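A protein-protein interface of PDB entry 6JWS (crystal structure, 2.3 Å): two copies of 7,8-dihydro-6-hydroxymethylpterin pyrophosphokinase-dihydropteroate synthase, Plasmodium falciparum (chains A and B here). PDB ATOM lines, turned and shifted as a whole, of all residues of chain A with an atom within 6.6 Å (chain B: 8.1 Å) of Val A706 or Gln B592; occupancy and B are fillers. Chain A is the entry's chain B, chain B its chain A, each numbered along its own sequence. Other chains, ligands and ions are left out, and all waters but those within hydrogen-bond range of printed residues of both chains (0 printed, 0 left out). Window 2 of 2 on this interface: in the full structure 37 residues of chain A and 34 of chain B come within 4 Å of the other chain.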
ATOM      1  N   THR A 701      -3.178  20.953  -9.819  1.00  0.00           N
ATOM      2  CA  THR A 701      -2.512  22.131  -9.283  1.00  0.00           C
ATOM      3  C   THR A 701      -1.927  21.843  -7.895  1.00  0.00           C
ATOM      4  O   THR A 701      -0.810  22.281  -7.589  1.00  0.00           O
ATOM      5  CB  THR A 701      -3.439  23.362  -9.285  1.00  0.00           C
ATOM      6  OG1 THR A 701      -3.869  23.627 -10.628  1.00  0.00           O
ATOM      7  CG2 THR A 701      -2.730  24.604  -8.793  1.00  0.00           C
ATOM      8  N   LYS A 702      -2.683  21.111  -7.056  1.00  0.00           N
ATOM      9  CA  LYS A 702      -2.246  20.806  -5.704  1.00  0.00           C
ATOM     10  C   LYS A 702      -1.038  19.875  -5.736  1.00  0.00           C
ATOM     11  O   LYS A 702      -0.095  20.077  -4.979  1.00  0.00           O
ATOM     12  CB  LYS A 702      -3.350  20.171  -4.855  1.00  0.00           C
ATOM     13  CG  LYS A 702      -3.898  21.089  -3.780  1.00  0.00           C
ATOM     14  CD  LYS A 702      -3.085  21.104  -2.506  1.00  0.00           C
ATOM     15  CE  LYS A 702      -3.669  22.070  -1.486  1.00  0.00           C
ATOM     16  NZ  LYS A 702      -2.745  22.318  -0.354  1.00  0.00           N
ATOM     17  N   ILE A 703      -1.091  18.847  -6.589  1.00  0.00           N
ATOM     18  CA  ILE A 703       0.028  17.934  -6.686  1.00  0.00           C
ATOM     19  C   ILE A 703       1.281  18.691  -7.137  1.00  0.00           C
ATOM     20  O   ILE A 703       2.382  18.369  -6.685  1.00  0.00           O
ATOM     21  CB  ILE A 703      -0.317  16.739  -7.592  1.00  0.00           C
ATOM     22  CG1 ILE A 703      -1.453  15.904  -6.997  1.00  0.00           C
ATOM     23  CG2 ILE A 703       0.929  15.906  -7.878  1.00  0.00           C
ATOM     24  CD1 ILE A 703      -1.951  14.799  -7.910  1.00  0.00           C
ATOM     25  N   ASP A 704       1.102  19.732  -7.970  1.00  0.00           N
ATOM     26  CA  ASP A 704       2.223  20.466  -8.543  1.00  0.00           C
ATOM     27  C   ASP A 704       2.809  21.501  -7.588  1.00  0.00           C
ATOM     28  O   ASP A 704       3.909  21.982  -7.835  1.00  0.00           O
ATOM     29  CB  ASP A 704       1.821  21.213  -9.813  1.00  0.00           C
ATOM     30  CG  ASP A 704       2.317  20.568 -11.090  1.00  0.00           C
ATOM     31  OD1 ASP A 704       3.102  19.600 -11.002  1.00  0.00           O
ATOM     32  OD2 ASP A 704       1.916  21.046 -12.165  1.00  0.00           O
ATOM     33  N   GLN A 705       2.072  21.899  -6.545  1.00  0.00           N
ATOM     34  CA  GLN A 705       2.604  22.916  -5.647  1.00  0.00           C
ATOM     35  C   GLN A 705       3.466  22.258  -4.570  1.00  0.00           C
ATOM     36  O   GLN A 705       2.979  21.875  -3.511  1.00  0.00           O
ATOM     37  CB  GLN A 705       1.527  23.884  -5.143  1.00  0.00           C
ATOM     38  CG  GLN A 705       0.550  23.272  -4.157  1.00  0.00           C
ATOM     39  CD  GLN A 705      -0.060  24.261  -3.191  1.00  0.00           C
ATOM     40  OE1 GLN A 705      -0.024  25.471  -3.399  1.00  0.00           O
ATOM     41  NE2 GLN A 705      -0.640  23.743  -2.117  1.00  0.00           N
ATOM     42  N   VAL A 706       4.754  22.090  -4.883  1.00  0.00           N
ATOM     43  CA  VAL A 706       5.715  21.516  -3.955  1.00  0.00           C
ATOM     44  C   VAL A 706       6.077  22.575  -2.912  1.00  0.00           C
ATOM     45  O   VAL A 706       6.303  23.736  -3.250  1.00  0.00           O
ATOM     46  CB  VAL A 706       6.946  20.951  -4.694  1.00  0.00           C
ATOM     47  CG1 VAL A 706       6.626  19.622  -5.369  1.00  0.00           C
ATOM     48  CG2 VAL A 706       7.501  21.935  -5.718  1.00  0.00           C
ATOM     49  N   LYS A 707       6.086  22.175  -1.636  1.00  0.00           N
ATOM     50  CA  LYS A 707       6.468  23.098  -0.579  1.00  0.00           C
ATOM     51  C   LYS A 707       7.939  23.511  -0.736  1.00  0.00           C
ATOM     52  O   LYS A 707       8.236  24.705  -0.767  1.00  0.00           O
ATOM     53  CB  LYS A 707       6.072  22.552   0.796  1.00  0.00           C
ATOM     54  CG  LYS A 707       5.424  23.577   1.717  1.00  0.00           C
ATOM     55  CD  LYS A 707       4.857  22.992   2.997  1.00  0.00           C
ATOM     56  CE  LYS A 707       4.778  24.001   4.126  1.00  0.00           C
ATOM     57  NZ  LYS A 707       6.118  24.405   4.617  1.00  0.00           N
ATOM     58  N   ASP A 708       8.846  22.526  -0.885  1.00  0.00           N
ATOM     59  CA  ASP A 708      10.273  22.782  -1.074  1.00  0.00           C
ATOM     60  C   ASP A 708      10.787  22.074  -2.332  1.00  0.00           C
ATOM     61  O   ASP A 708      10.769  20.845  -2.402  1.00  0.00           O
ATOM     62  CB  ASP A 708      11.069  22.405   0.184  1.00  0.00           C
ATOM     63  CG  ASP A 708      12.587  22.561   0.091  1.00  0.00           C
ATOM     64  OD1 ASP A 708      13.085  23.082  -0.942  1.00  0.00           O
ATOM     65  OD2 ASP A 708      13.268  22.161   1.064  1.00  0.00           O
ATOM     66  N   PRO A 709      11.287  22.817  -3.354  1.00  0.00           N
ATOM     67  CA  PRO A 709      11.722  22.214  -4.619  1.00  0.00           C
ATOM     68  C   PRO A 709      13.021  21.404  -4.627  1.00  0.00           C
ATOM     69  O   PRO A 709      13.410  20.876  -5.668  1.00  0.00           O
ATOM     70  CB  PRO A 709      11.854  23.415  -5.577  1.00  0.00           C
ATOM     71  CG  PRO A 709      12.127  24.595  -4.665  1.00  0.00           C
ATOM     72  CD  PRO A 709      11.392  24.287  -3.374  1.00  0.00           C
ATOM     73  N   SER A 711      13.578  19.353  -1.708  1.00  0.00           N
ATOM     74  CA  SER A 711      13.283  18.431  -0.619  1.00  0.00           C
ATOM     75  C   SER A 711      13.482  16.974  -1.036  1.00  0.00           C
ATOM     76  O   SER A 711      13.963  16.181  -0.239  1.00  0.00           O
ATOM     77  CB  SER A 711      11.916  18.667  -0.007  1.00  0.00           C
ATOM     78  OG  SER A 711      10.916  17.900  -0.664  1.00  0.00           O
ATOM     79  N   VAL B 548       8.395  10.349   3.319  1.00  0.00           N
ATOM     80  CA  VAL B 548       8.487   9.639   2.056  1.00  0.00           C
ATOM     81  C   VAL B 548       9.390   8.411   2.191  1.00  0.00           C
ATOM     82  O   VAL B 548       9.036   7.334   1.707  1.00  0.00           O
ATOM     83  CB  VAL B 548       8.925  10.578   0.913  1.00  0.00           C
ATOM     84  CG1 VAL B 548       9.319   9.799  -0.335  1.00  0.00           C
ATOM     85  CG2 VAL B 548       7.853  11.607   0.586  1.00  0.00           C
ATOM     86  N   ILE B 576       1.514   2.785  -0.639  1.00  0.00           N
ATOM     87  CA  ILE B 576       1.907   3.814   0.315  1.00  0.00           C
ATOM     88  C   ILE B 576       0.797   4.068   1.330  1.00  0.00           C
ATOM     89  O   ILE B 576       1.018   4.827   2.266  1.00  0.00           O
ATOM     90  CB  ILE B 576       2.194   5.145  -0.401  1.00  0.00           C
ATOM     91  CG1 ILE B 576       0.980   5.539  -1.252  1.00  0.00           C
ATOM     92  CG2 ILE B 576       3.501   5.059  -1.177  1.00  0.00           C
ATOM     93  CD1 ILE B 576       1.268   6.494  -2.368  1.00  0.00           C
ATOM     94  N   LEU B 578      -2.378   5.791   1.050  1.00  0.00           N
ATOM     95  CA  LEU B 578      -2.989   7.116   1.071  1.00  0.00           C
ATOM     96  C   LEU B 578      -4.157   7.135   2.058  1.00  0.00           C
ATOM     97  O   LEU B 578      -4.949   6.190   2.102  1.00  0.00           O
ATOM     98  CB  LEU B 578      -3.479   7.477  -0.339  1.00  0.00           C
ATOM     99  CG  LEU B 578      -2.382   7.611  -1.399  1.00  0.00           C
ATOM    100  CD1 LEU B 578      -2.964   7.819  -2.811  1.00  0.00           C
ATOM    101  CD2 LEU B 578      -1.408   8.730  -1.055  1.00  0.00           C
ATOM    102  N   ASP B 585      -2.175  16.775   3.453  1.00  0.00           N
ATOM    103  CA  ASP B 585      -0.961  17.293   2.826  1.00  0.00           C
ATOM    104  C   ASP B 585       0.083  16.180   2.721  1.00  0.00           C
ATOM    105  O   ASP B 585       0.851  16.163   1.780  1.00  0.00           O
ATOM    106  CB  ASP B 585      -0.385  18.545   3.515  1.00  0.00           C
ATOM    107  CG  ASP B 585      -1.197  19.831   3.336  1.00  0.00           C
ATOM    108  OD1 ASP B 585      -2.010  19.917   2.369  1.00  0.00           O
ATOM    109  OD2 ASP B 585      -1.034  20.754   4.176  1.00  0.00           O
ATOM    110  N   GLN B 586       0.095  15.238   3.674  1.00  0.00           N
ATOM    111  CA  GLN B 586       1.030  14.122   3.652  1.00  0.00           C
ATOM    112  C   GLN B 586       0.641  13.122   2.560  1.00  0.00           C
ATOM    113  O   GLN B 586       1.495  12.616   1.841  1.00  0.00           O
ATOM    114  CB  GLN B 586       1.055  13.468   5.030  1.00  0.00           C
ATOM    115  CG  GLN B 586       1.711  14.323   6.107  1.00  0.00           C
ATOM    116  CD  GLN B 586       1.634  13.671   7.469  1.00  0.00           C
ATOM    117  OE1 GLN B 586       0.617  13.092   7.853  1.00  0.00           O
ATOM    118  NE2 GLN B 586       2.719  13.765   8.215  1.00  0.00           N
ATOM    119  N   SER B 587      -0.658  12.882   2.392  1.00  0.00           N
ATOM    120  CA  SER B 587      -1.173  12.090   1.279  1.00  0.00           C
ATOM    121  C   SER B 587      -0.736  12.660  -0.081  1.00  0.00           C
ATOM    122  O   SER B 587      -0.195  11.926  -0.918  1.00  0.00           O
ATOM    123  CB  SER B 587      -2.653  11.982   1.381  1.00  0.00           C
ATOM    124  OG  SER B 587      -3.042  11.021   2.343  1.00  0.00           O
ATOM    125  N   ILE B 588      -0.901  13.977  -0.274  1.00  0.00           N
ATOM    126  CA  ILE B 588      -0.421  14.712  -1.449  1.00  0.00           C
ATOM    127  C   ILE B 588       1.093  14.572  -1.630  1.00  0.00           C
ATOM    128  O   ILE B 588       1.575  14.317  -2.746  1.00  0.00           O
ATOM    129  CB  ILE B 588      -0.883  16.194  -1.422  1.00  0.00           C
ATOM    130  CG1 ILE B 588      -2.396  16.302  -1.603  1.00  0.00           C
ATOM    131  CG2 ILE B 588      -0.172  17.039  -2.461  1.00  0.00           C
ATOM    132  CD1 ILE B 588      -3.000  17.390  -0.758  1.00  0.00           C
ATOM    133  N   LYS B 589       1.843  14.743  -0.540  1.00  0.00           N
ATOM    134  CA  LYS B 589       3.300  14.678  -0.581  1.00  0.00           C
ATOM    135  C   LYS B 589       3.792  13.302  -1.071  1.00  0.00           C
ATOM    136  O   LYS B 589       4.775  13.198  -1.808  1.00  0.00           O
ATOM    137  CB  LYS B 589       3.794  14.901   0.849  1.00  0.00           C
ATOM    138  CG  LYS B 589       5.024  15.771   1.026  1.00  0.00           C
ATOM    139  CD  LYS B 589       6.306  15.041   0.957  1.00  0.00           C
ATOM    140  CE  LYS B 589       7.451  15.949   1.350  1.00  0.00           C
ATOM    141  NZ  LYS B 589       7.447  16.197   2.816  1.00  0.00           N
ATOM    142  N   LEU B 590       3.157  12.235  -0.588  1.00  0.00           N
ATOM    143  CA  LEU B 590       3.434  10.889  -1.061  1.00  0.00           C
ATOM    144  C   LEU B 590       3.228  10.809  -2.578  1.00  0.00           C
ATOM    145  O   LEU B 590       4.091  10.309  -3.299  1.00  0.00           O
ATOM    146  CB  LEU B 590       2.529   9.909  -0.298  1.00  0.00           C
ATOM    147  CG  LEU B 590       2.933   9.695   1.165  1.00  0.00           C
ATOM    148  CD1 LEU B 590       1.915   8.819   1.893  1.00  0.00           C
ATOM    149  CD2 LEU B 590       4.329   9.082   1.253  1.00  0.00           C
ATOM    150  N   LEU B 591       2.089  11.312  -3.060  1.00  0.00           N
ATOM    151  CA  LEU B 591       1.813  11.321  -4.495  1.00  0.00           C
ATOM    152  C   LEU B 591       2.882  12.114  -5.245  1.00  0.00           C
ATOM    153  O   LEU B 591       3.374  11.659  -6.268  1.00  0.00           O
ATOM    154  CB  LEU B 591       0.422  11.913  -4.758  1.00  0.00           C
ATOM    155  CG  LEU B 591      -0.725  10.927  -4.581  1.00  0.00           C
ATOM    156  CD1 LEU B 591      -2.060  11.623  -4.788  1.00  0.00           C
ATOM    157  CD2 LEU B 591      -0.545   9.753  -5.549  1.00  0.00           C
ATOM    158  N   GLN B 592       3.239  13.293  -4.732  1.00  0.00           N
ATOM    159  CA  GLN B 592       4.229  14.132  -5.381  1.00  0.00           C
ATOM    160  C   GLN B 592       5.551  13.383  -5.519  1.00  0.00           C
ATOM    161  O   GLN B 592       6.331  13.669  -6.424  1.00  0.00           O
ATOM    162  CB  GLN B 592       4.474  15.402  -4.566  1.00  0.00           C
ATOM    163  CG  GLN B 592       3.318  16.383  -4.596  1.00  0.00           C
ATOM    164  CD  GLN B 592       3.573  17.566  -3.687  1.00  0.00           C
ATOM    165  OE1 GLN B 592       4.265  17.452  -2.676  1.00  0.00           O
ATOM    166  NE2 GLN B 592       3.028  18.721  -4.046  1.00  0.00           N
ATOM    167  N   ASN B 593       5.799  12.434  -4.613  1.00  0.00           N
ATOM    168  CA  ASN B 593       7.101  11.793  -4.512  1.00  0.00           C
ATOM    169  C   ASN B 593       6.982  10.316  -4.861  1.00  0.00           C
ATOM    170  O   ASN B 593       7.785   9.500  -4.421  1.00  0.00           O
ATOM    171  CB  ASN B 593       7.713  12.011  -3.126  1.00  0.00           C
ATOM    172  CG  ASN B 593       8.133  13.452  -2.958  1.00  0.00           C
ATOM    173  OD1 ASN B 593       9.172  13.850  -3.483  1.00  0.00           O
ATOM    174  ND2 ASN B 593       7.318  14.248  -2.284  1.00  0.00           N
ATOM    175  N   ILE B 594       6.003   9.998  -5.696  1.00  0.00           N
ATOM    176  CA  ILE B 594       5.703   8.631  -6.084  1.00  0.00           C
ATOM    177  C   ILE B 594       6.847   8.055  -6.930  1.00  0.00           C
ATOM    178  O   ILE B 594       6.977   6.841  -7.032  1.00  0.00           O
ATOM    179  CB  ILE B 594       4.312   8.627  -6.776  1.00  0.00           C
ATOM    180  CG1 ILE B 594       3.490   7.355  -6.552  1.00  0.00           C
ATOM    181  CG2 ILE B 594       4.380   9.034  -8.245  1.00  0.00           C
ATOM    182  CD1 ILE B 594       3.220   7.047  -5.109  1.00  0.00           C
ATOM    183  N   HIS B 595       7.712   8.916  -7.498  1.00  0.00           N
ATOM    184  CA  HIS B 595       8.853   8.466  -8.293  1.00  0.00           C
ATOM    185  C   HIS B 595       9.791   7.565  -7.480  1.00  0.00           C
ATOM    186  O   HIS B 595      10.581   6.821  -8.067  1.00  0.00           O
ATOM    187  CB  HIS B 595       9.637   9.657  -8.908  1.00  0.00           C
ATOM    188  CG  HIS B 595      10.352  10.454  -7.854  1.00  0.00           C
ATOM    189  ND1 HIS B 595       9.742  11.511  -7.175  1.00  0.00           N
ATOM    190  CD2 HIS B 595      11.573  10.284  -7.288  1.00  0.00           C
ATOM    191  CE1 HIS B 595      10.567  11.976  -6.252  1.00  0.00           C
ATOM    192  NE2 HIS B 595      11.700  11.210  -6.280  1.00  0.00           N
ATOM    193  N   VAL B 596       9.733   7.622  -6.135  1.00  0.00           N
ATOM    194  CA  VAL B 596      10.608   6.760  -5.339  1.00  0.00           C
ATOM    195  C   VAL B 596      10.266   5.273  -5.519  1.00  0.00           C
ATOM    196  O   VAL B 596      11.068   4.436  -5.118  1.00  0.00           O
ATOM    197  CB  VAL B 596      10.679   7.163  -3.848  1.00  0.00           C
ATOM    198  CG1 VAL B 596      11.134   8.625  -3.654  1.00  0.00           C
ATOM    199  CG2 VAL B 596       9.359   6.865  -3.113  1.00  0.00           C
ATOM    200  N   TYR B 676      -2.510  11.553 -13.440  1.00  0.00           N
ATOM    201  CA  TYR B 676      -1.196  11.625 -12.823  1.00  0.00           C
ATOM    202  C   TYR B 676      -0.548  10.244 -12.767  1.00  0.00           C
ATOM    203  O   TYR B 676       0.617  10.097 -13.125  1.00  0.00           O
ATOM    204  CB  TYR B 676      -1.330  12.261 -11.440  1.00  0.00           C
ATOM    205  CG  TYR B 676      -0.025  12.438 -10.718  1.00  0.00           C
ATOM    206  CD1 TYR B 676       0.895  13.400 -11.120  1.00  0.00           C
ATOM    207  CD2 TYR B 676       0.259  11.664  -9.605  1.00  0.00           C
ATOM    208  CE1 TYR B 676       2.082  13.590 -10.435  1.00  0.00           C
ATOM    209  CE2 TYR B 676       1.440  11.841  -8.907  1.00  0.00           C
ATOM    210  CZ  TYR B 676       2.351  12.791  -9.328  1.00  0.00           C
ATOM    211  OH  TYR B 676       3.494  12.943  -8.613  1.00  0.00           O
ATOM    212  N   LYS B 680       2.885   8.748 -14.309  1.00  0.00           N
ATOM    213  CA  LYS B 680       3.926   8.348 -13.373  1.00  0.00           C
ATOM    214  C   LYS B 680       4.133   6.845 -13.502  1.00  0.00           C
ATOM    215  O   LYS B 680       4.991   6.283 -12.830  1.00  0.00           O
ATOM    216  CB  LYS B 680       3.557   8.755 -11.938  1.00  0.00           C
ATOM    217  CG  LYS B 680       3.679  10.243 -11.654  1.00  0.00           C
ATOM    218  CD  LYS B 680       5.125  10.686 -11.723  1.00  0.00           C
ATOM    219  CE  LYS B 680       5.362  12.173 -11.879  1.00  0.00           C
ATOM    220  NZ  LYS B 680       6.664  12.539 -11.255  1.00  0.00           N
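OD1 of Asp B585 is in salt-bridge range of NZ of Lys A702 (3.7 Å). The backbone carbonyl oxygen (O) of Gln A705 is in hydrogen-bond range of the side-chain amide nitrogen (NE2) of Gln B592. The side-chain amide nitrogen of Gln B592 lies within hydrogen-bond range of the backbone carbonyl oxygen of Ile A703, 2.7 Å away.
Of the 17 printed residues of chain B, 4 touch a printed residue of chain A. Hydrophobic or aromatic side chains of chain B that line the printed part of chain A: Ile B588 and Tyr B676.
Among the printed residues, pairs that only touch across the chains: Lys A702 with Gln B592 (3.5 Å), Ile A703 with Tyr B676 (3.6 Å), Val A706 with Gln B592 (3.9 Å) and Lys A702 with Ile B588 (3.9 Å).
Of the printed residues of chain B, Gln A705 touches Gln B592. Of the printed residues of chain B, Val A706 touches Gln B592 (3.9 Å). Of the printed residues of chain A, Asp B585 touches Lys A702. Of the printed residues of chain A, Ile B588 touches Lys A702 (3.9 Å). Printed residues of chain A within 4 Å of Tyr B676: Ile A703. The nearest residue of chain B that does not touch Val A706 is Asn B593 (6.2 Å). The nearest residue of chain A that does not touch Gln B592 is Asp A704 (4.5 Å).
NZ of Lys A702 lies close to NE2 of Gln A705, 3.1 Å away. The side-chain hydroxyl (OH) of Tyr B676 is in hydrogen-bond range of the backbone carbonyl oxygen (O) of Leu B591 (2.7 Å).
No position is printed for both chains.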
